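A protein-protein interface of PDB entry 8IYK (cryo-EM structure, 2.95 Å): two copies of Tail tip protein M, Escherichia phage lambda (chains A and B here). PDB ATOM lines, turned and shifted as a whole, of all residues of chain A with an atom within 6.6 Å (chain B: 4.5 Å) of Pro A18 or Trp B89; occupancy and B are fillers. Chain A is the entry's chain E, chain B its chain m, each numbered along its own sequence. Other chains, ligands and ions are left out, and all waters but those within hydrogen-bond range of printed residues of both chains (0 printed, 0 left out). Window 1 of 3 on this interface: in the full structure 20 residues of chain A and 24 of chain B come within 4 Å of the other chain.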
ATOM      1  N   VAL A  14     -21.000 -22.851  22.187  1.00  0.00           N
ATOM      2  CA  VAL A  14     -22.036 -22.271  23.031  1.00  0.00           C
ATOM      3  C   VAL A  14     -22.334 -20.883  22.482  1.00  0.00           C
ATOM      4  O   VAL A  14     -21.583 -19.932  22.720  1.00  0.00           O
ATOM      5  CB  VAL A  14     -21.608 -22.227  24.499  1.00  0.00           C
ATOM      6  CG1 VAL A  14     -22.811 -22.061  25.387  1.00  0.00           C
ATOM      7  CG2 VAL A  14     -20.854 -23.494  24.857  1.00  0.00           C
ATOM      8  N   ALA A  15     -23.437 -20.760  21.749  1.00  0.00           N
ATOM      9  CA  ALA A  15     -23.791 -19.525  21.062  1.00  0.00           C
ATOM     10  C   ALA A  15     -24.856 -18.774  21.848  1.00  0.00           C
ATOM     11  O   ALA A  15     -25.858 -19.364  22.266  1.00  0.00           O
ATOM     12  CB  ALA A  15     -24.288 -19.816  19.647  1.00  0.00           C
ATOM     13  N   SER A  16     -24.640 -17.472  22.041  1.00  0.00           N
ATOM     14  CA  SER A  16     -25.552 -16.637  22.818  1.00  0.00           C
ATOM     15  C   SER A  16     -26.482 -15.815  21.931  1.00  0.00           C
ATOM     16  O   SER A  16     -27.704 -15.958  22.019  1.00  0.00           O
ATOM     17  CB  SER A  16     -24.746 -15.718  23.743  1.00  0.00           C
ATOM     18  OG  SER A  16     -23.925 -16.475  24.613  1.00  0.00           O
ATOM     19  N   VAL A  17     -25.915 -14.969  21.071  1.00  0.00           N
ATOM     20  CA  VAL A  17     -26.618 -14.097  20.122  1.00  0.00           C
ATOM     21  C   VAL A  17     -27.904 -13.525  20.723  1.00  0.00           C
ATOM     22  O   VAL A  17     -29.014 -13.908  20.326  1.00  0.00           O
ATOM     23  CB  VAL A  17     -26.844 -14.820  18.775  1.00  0.00           C
ATOM     24  CG1 VAL A  17     -27.715 -16.081  18.894  1.00  0.00           C
ATOM     25  CG2 VAL A  17     -27.394 -13.854  17.722  1.00  0.00           C
ATOM     26  N   PRO A  18     -27.806 -12.612  21.686  1.00  0.00           N
ATOM     27  CA  PRO A  18     -29.015 -12.014  22.257  1.00  0.00           C
ATOM     28  C   PRO A  18     -29.729 -11.130  21.248  1.00  0.00           C
ATOM     29  O   PRO A  18     -29.117 -10.555  20.346  1.00  0.00           O
ATOM     30  CB  PRO A  18     -28.481 -11.191  23.431  1.00  0.00           C
ATOM     31  CG  PRO A  18     -27.121 -10.803  22.995  1.00  0.00           C
ATOM     32  CD  PRO A  18     -26.588 -11.983  22.223  1.00  0.00           C
ATOM     33  N   SER A  19     -31.044 -11.025  21.417  1.00  0.00           N
ATOM     34  CA  SER A  19     -31.887 -10.223  20.541  1.00  0.00           C
ATOM     35  C   SER A  19     -32.043  -8.830  21.138  1.00  0.00           C
ATOM     36  O   SER A  19     -32.446  -8.690  22.297  1.00  0.00           O
ATOM     37  CB  SER A  19     -33.253 -10.879  20.349  1.00  0.00           C
ATOM     38  OG  SER A  19     -34.128 -10.547  21.411  1.00  0.00           O
ATOM     39  N   VAL A  20     -31.726  -7.808  20.345  1.00  0.00           N
ATOM     40  CA  VAL A  20     -31.813  -6.422  20.781  1.00  0.00           C
ATOM     41  C   VAL A  20     -32.563  -5.617  19.730  1.00  0.00           C
ATOM     42  O   VAL A  20     -32.630  -5.987  18.556  1.00  0.00           O
ATOM     43  CB  VAL A  20     -30.423  -5.801  21.033  1.00  0.00           C
ATOM     44  CG1 VAL A  20     -29.811  -6.377  22.293  1.00  0.00           C
ATOM     45  CG2 VAL A  20     -29.516  -6.037  19.842  1.00  0.00           C
ATOM     46  N   ALA A  39     -33.463 -12.083  29.416  1.00  0.00           N
ATOM     47  CA  ALA A  39     -32.157 -12.526  28.938  1.00  0.00           C
ATOM     48  C   ALA A  39     -32.181 -13.140  27.544  1.00  0.00           C
ATOM     49  O   ALA A  39     -33.113 -12.917  26.764  1.00  0.00           O
ATOM     50  CB  ALA A  39     -31.558 -13.532  29.925  1.00  0.00           C
ATOM     51  N   ASN A  40     -31.135 -13.895  27.220  1.00  0.00           N
ATOM     52  CA  ASN A  40     -31.077 -14.729  26.033  1.00  0.00           C
ATOM     53  C   ASN A  40     -30.908 -16.182  26.459  1.00  0.00           C
ATOM     54  O   ASN A  40     -30.464 -16.475  27.572  1.00  0.00           O
ATOM     55  CB  ASN A  40     -29.938 -14.302  25.101  1.00  0.00           C
ATOM     56  CG  ASN A  40     -28.646 -14.069  25.842  1.00  0.00           C
ATOM     57  OD1 ASN A  40     -28.654 -13.644  26.996  1.00  0.00           O
ATOM     58  ND2 ASN A  40     -27.525 -14.345  25.188  1.00  0.00           N
ATOM     59  N   LEU A  41     -31.266 -17.094  25.558  1.00  0.00           N
ATOM     60  CA  LEU A  41     -31.440 -18.484  25.955  1.00  0.00           C
ATOM     61  C   LEU A  41     -30.179 -19.325  25.790  1.00  0.00           C
ATOM     62  O   LEU A  41     -29.943 -20.222  26.606  1.00  0.00           O
ATOM     63  CB  LEU A  41     -32.598 -19.104  25.173  1.00  0.00           C
ATOM     64  CG  LEU A  41     -33.974 -18.704  25.712  1.00  0.00           C
ATOM     65  CD1 LEU A  41     -35.072 -19.549  25.090  1.00  0.00           C
ATOM     66  CD2 LEU A  41     -34.006 -18.815  27.230  1.00  0.00           C
ATOM     67  N   LYS A  42     -29.389 -19.082  24.739  1.00  0.00           N
ATOM     68  CA  LYS A  42     -28.089 -19.729  24.544  1.00  0.00           C
ATOM     69  C   LYS A  42     -28.248 -21.186  24.116  1.00  0.00           C
ATOM     70  O   LYS A  42     -29.057 -21.922  24.688  1.00  0.00           O
ATOM     71  CB  LYS A  42     -27.246 -19.614  25.820  1.00  0.00           C
ATOM     72  CG  LYS A  42     -25.881 -20.256  25.764  1.00  0.00           C
ATOM     73  CD  LYS A  42     -25.140 -20.070  27.084  1.00  0.00           C
ATOM     74  CE  LYS A  42     -25.428 -18.718  27.719  1.00  0.00           C
ATOM     75  NZ  LYS A  42     -24.722 -17.611  27.020  1.00  0.00           N
ATOM     76  N   TYR A  77     -20.186 -26.318  31.185  1.00  0.00           N
ATOM     77  CA  TYR A  77     -19.728 -24.967  30.899  1.00  0.00           C
ATOM     78  C   TYR A  77     -19.881 -24.042  32.094  1.00  0.00           C
ATOM     79  O   TYR A  77     -18.913 -23.387  32.495  1.00  0.00           O
ATOM     80  CB  TYR A  77     -20.501 -24.418  29.692  1.00  0.00           C
ATOM     81  CG  TYR A  77     -19.907 -23.177  29.080  1.00  0.00           C
ATOM     82  CD1 TYR A  77     -18.614 -22.773  29.383  1.00  0.00           C
ATOM     83  CD2 TYR A  77     -20.635 -22.419  28.182  1.00  0.00           C
ATOM     84  CE1 TYR A  77     -18.072 -21.643  28.814  1.00  0.00           C
ATOM     85  CE2 TYR A  77     -20.101 -21.298  27.606  1.00  0.00           C
ATOM     86  CZ  TYR A  77     -18.821 -20.909  27.925  1.00  0.00           C
ATOM     87  OH  TYR A  77     -18.294 -19.777  27.351  1.00  0.00           O
ATOM     88  N   GLU B  59     -18.296 -14.679  30.390  1.00  0.00           N
ATOM     89  CA  GLU B  59     -19.654 -14.714  29.868  1.00  0.00           C
ATOM     90  C   GLU B  59     -20.619 -13.922  30.732  1.00  0.00           C
ATOM     91  O   GLU B  59     -21.598 -13.393  30.212  1.00  0.00           O
ATOM     92  CB  GLU B  59     -20.155 -16.145  29.721  1.00  0.00           C
ATOM     93  CG  GLU B  59     -21.075 -16.304  28.527  1.00  0.00           C
ATOM     94  CD  GLU B  59     -20.829 -17.584  27.786  1.00  0.00           C
ATOM     95  OE1 GLU B  59     -20.960 -17.604  26.545  1.00  0.00           O
ATOM     96  OE2 GLU B  59     -20.501 -18.574  28.460  1.00  0.00           O
ATOM     97  N   LEU B  62     -20.151 -10.427  29.415  1.00  0.00           N
ATOM     98  CA  LEU B  62     -20.749 -10.220  28.100  1.00  0.00           C
ATOM     99  C   LEU B  62     -22.267 -10.363  28.135  1.00  0.00           C
ATOM    100  O   LEU B  62     -22.966  -9.759  27.315  1.00  0.00           O
ATOM    101  CB  LEU B  62     -20.137 -11.190  27.091  1.00  0.00           C
ATOM    102  CG  LEU B  62     -18.784 -10.753  26.527  1.00  0.00           C
ATOM    103  CD1 LEU B  62     -18.083 -11.912  25.841  1.00  0.00           C
ATOM    104  CD2 LEU B  62     -18.957  -9.585  25.573  1.00  0.00           C
ATOM    105  N   GLU B  63     -22.791 -11.149  29.074  1.00  0.00           N
ATOM    106  CA  GLU B  63     -24.218 -11.419  29.171  1.00  0.00           C
ATOM    107  C   GLU B  63     -24.957 -10.263  29.826  1.00  0.00           C
ATOM    108  O   GLU B  63     -26.082  -9.940  29.432  1.00  0.00           O
ATOM    109  CB  GLU B  63     -24.434 -12.702  29.972  1.00  0.00           C
ATOM    110  CG  GLU B  63     -25.741 -13.424  29.723  1.00  0.00           C
ATOM    111  CD  GLU B  63     -25.569 -14.590  28.767  1.00  0.00           C
ATOM    112  OE1 GLU B  63     -24.504 -15.238  28.811  1.00  0.00           O
ATOM    113  OE2 GLU B  63     -26.497 -14.873  27.983  1.00  0.00           O
ATOM    114  N   GLY B  66     -25.423  -7.669  27.188  1.00  0.00           N
ATOM    115  CA  GLY B  66     -26.470  -8.272  26.387  1.00  0.00           C
ATOM    116  C   GLY B  66     -26.832  -7.561  25.101  1.00  0.00           C
ATOM    117  O   GLY B  66     -28.016  -7.353  24.820  1.00  0.00           O
ATOM    118  N   GLY B  67     -25.841  -7.187  24.313  1.00  0.00           N
ATOM    119  CA  GLY B  67     -26.096  -6.529  23.036  1.00  0.00           C
ATOM    120  C   GLY B  67     -26.160  -5.024  23.107  1.00  0.00           C
ATOM    121  O   GLY B  67     -25.492  -4.335  22.339  1.00  0.00           O
ATOM    122  N   CYS B  86     -20.924  -5.718  21.712  1.00  0.00           N
ATOM    123  CA  CYS B  86     -20.796  -7.093  21.249  1.00  0.00           C
ATOM    124  C   CYS B  86     -22.177  -7.720  21.152  1.00  0.00           C
ATOM    125  O   CYS B  86     -23.070  -7.394  21.939  1.00  0.00           O
ATOM    126  CB  CYS B  86     -19.912  -7.920  22.186  1.00  0.00           C
ATOM    127  SG  CYS B  86     -19.726  -9.644  21.689  1.00  0.00           S
ATOM    128  N   ALA B  87     -22.353  -8.620  20.183  1.00  0.00           N
ATOM    129  CA  ALA B  87     -23.661  -9.202  19.925  1.00  0.00           C
ATOM    130  C   ALA B  87     -23.674 -10.711  19.723  1.00  0.00           C
ATOM    131  O   ALA B  87     -24.758 -11.299  19.778  1.00  0.00           O
ATOM    132  CB  ALA B  87     -24.303  -8.542  18.696  1.00  0.00           C
ATOM    133  N   LYS B  88     -22.535 -11.358  19.468  1.00  0.00           N
ATOM    134  CA  LYS B  88     -22.536 -12.801  19.247  1.00  0.00           C
ATOM    135  C   LYS B  88     -21.753 -13.561  20.309  1.00  0.00           C
ATOM    136  O   LYS B  88     -22.338 -14.378  21.029  1.00  0.00           O
ATOM    137  CB  LYS B  88     -21.977 -13.098  17.851  1.00  0.00           C
ATOM    138  CG  LYS B  88     -22.436 -12.116  16.782  1.00  0.00           C
ATOM    139  CD  LYS B  88     -23.442 -12.737  15.827  1.00  0.00           C
ATOM    140  CE  LYS B  88     -22.918 -14.035  15.235  1.00  0.00           C
ATOM    141  NZ  LYS B  88     -23.956 -14.735  14.430  1.00  0.00           N
ATOM    142  N   TRP B  89     -20.456 -13.297  20.440  1.00  0.00           N
ATOM    143  CA  TRP B  89     -19.553 -13.934  21.407  1.00  0.00           C
ATOM    144  C   TRP B  89     -19.820 -15.438  21.567  1.00  0.00           C
ATOM    145  O   TRP B  89     -20.175 -15.939  22.632  1.00  0.00           O
ATOM    146  CB  TRP B  89     -19.546 -13.173  22.744  1.00  0.00           C
ATOM    147  CG  TRP B  89     -20.640 -13.399  23.761  1.00  0.00           C
ATOM    148  CD1 TRP B  89     -20.647 -14.316  24.774  1.00  0.00           C
ATOM    149  CD2 TRP B  89     -21.823 -12.614  23.931  1.00  0.00           C
ATOM    150  NE1 TRP B  89     -21.788 -14.191  25.521  1.00  0.00           N
ATOM    151  CE2 TRP B  89     -22.525 -13.147  25.030  1.00  0.00           C
ATOM    152  CE3 TRP B  89     -22.371 -11.526  23.247  1.00  0.00           C
ATOM    153  CZ2 TRP B  89     -23.741 -12.632  25.456  1.00  0.00           C
ATOM    154  CZ3 TRP B  89     -23.577 -11.017  23.672  1.00  0.00           C
ATOM    155  CH2 TRP B  89     -24.249 -11.569  24.767  1.00  0.00           C
ATOM    156  N   SER B  90     -19.626 -16.166  20.472  1.00  0.00           N
ATOM    157  CA  SER B  90     -19.650 -17.618  20.557  1.00  0.00           C
ATOM    158  C   SER B  90     -18.456 -18.120  21.368  1.00  0.00           C
ATOM    159  O   SER B  90     -17.462 -17.419  21.557  1.00  0.00           O
ATOM    160  CB  SER B  90     -19.635 -18.243  19.164  1.00  0.00           C
ATOM    161  OG  SER B  90     -19.286 -19.615  19.225  1.00  0.00           O
ATOM    162  N   SER B  91     -18.564 -19.352  21.862  1.00  0.00           N
ATOM    163  CA  SER B  91     -17.514 -19.925  22.692  1.00  0.00           C
ATOM    164  C   SER B  91     -17.355 -21.408  22.394  1.00  0.00           C
ATOM    165  O   SER B  91     -18.300 -22.079  21.973  1.00  0.00           O
ATOM    166  CB  SER B  91     -17.804 -19.725  24.182  1.00  0.00           C
ATOM    167  OG  SER B  91     -17.275 -20.793  24.946  1.00  0.00           O
ATOM    168  N   SER B 101     -15.027 -16.214  20.607  1.00  0.00           N
ATOM    169  CA  SER B 101     -15.032 -15.491  19.341  1.00  0.00           C
ATOM    170  C   SER B 101     -16.134 -14.445  19.420  1.00  0.00           C
ATOM    171  O   SER B 101     -17.321 -14.783  19.352  1.00  0.00           O
ATOM    172  CB  SER B 101     -15.255 -16.440  18.165  1.00  0.00           C
ATOM    173  OG  SER B 101     -14.643 -17.696  18.400  1.00  0.00           O
ATOM    174  N   ALA B 102     -15.747 -13.180  19.567  1.00  0.00           N
ATOM    175  CA  ALA B 102     -16.695 -12.092  19.728  1.00  0.00           C
ATOM    176  C   ALA B 102     -16.421 -11.026  18.678  1.00  0.00           C
ATOM    177  O   ALA B 102     -15.337 -10.962  18.096  1.00  0.00           O
ATOM    178  CB  ALA B 102     -16.621 -11.482  21.133  1.00  0.00           C
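The side-chain hydroxyl (OG) of Ser A16 is in hydrogen-bond range of the side-chain amino group (NZ) of Lys A42 (2.8 Å). The backbone carbonyl oxygen (O) of Ser B90 sits at hydrogen-bond distance from the backbone NH (N) of Ser B101, 2.9 Å away.
No position is printed for both chains. Of the 17 pairs that touch across the chains among the printed residues, none has its exchanged pair printed and touching as well.
Pro A18 touches just these residues of chain B: Gly B66, Ala B87 and Trp B89. Ser A19 touches none of the printed residues of chain B. Of the printed residues of chain B, Lys A42 touches Glu B59 and Glu B63. Of the printed residues of chain A, Glu B59 touches Ser A16, Lys A42 and Tyr A77. Printed residues of chain A within 4 Å of Glu B63: Asn A40 (2.7 Å) and Lys A42 (3.0 Å). Printed residues of chain A within 4 Å of Gly B67: Val A20 (3.8 Å). Trp B89 touches just these residues of chain A: Ser A16 and Pro A18. Of the printed residues of chain A, Ser B90 touches Val A14 (3.7 Å). Ala B102 touches none of the printed residues of chain A.
Ser B90 touches Val A14 (CA to O, 3.7 Å). Glu B59 touches Ser A16. Ser A16 touches Lys B88. Ala B87 touches Val A17. N of Val A17 touches O of Lys B88, 3.6 Å away. Gly B66 touches Pro A18. Pro A18 touches Ala B87 (CD to O, 3.1 Å). CH2 of Trp B89 touches CG of Pro A18, at 3.5 Å. Val A20 touches Gly B66 (CG1 to O, 3.2 Å). Val A20 touches Gly B67.
Hydrophobic or aromatic side chains of chain B that line the printed part of chain A: Trp B89. Among the printed residues, 17 pairs touch across the chains.
The side-chain carboxylate (OE2) of Glu B63 sits close to the side-chain amide oxygen (OD1) of Asn A40 (2.7 Å). OE2 of Glu B59 lies within hydrogen-bond range of OH of Tyr A77 (2.7 Å). The side-chain carboxylate (OE1) of Glu B63 lies within salt-bridge range of the side-chain amino group (NZ) of Lys A42 (3.0 Å). The indole nitrogen (NE1) of Trp B89 sits at hydrogen-bond distance from the side-chain hydroxyl (OG) of Ser A16 (3.3 Å). The backbone carbonyl oxygen of Ser B91 is in hydrogen-bond range of the backbone NH of Val A14 (2.8 Å). The side-chain carboxylate of Glu B59 is in salt-bridge range of the side-chain amino group of Lys A42. The side-chain hydroxyl (OH) of Tyr A77 is in hydrogen-bond range of the side-chain hydroxyl (OG) of Ser B91, at 2.8 Å.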
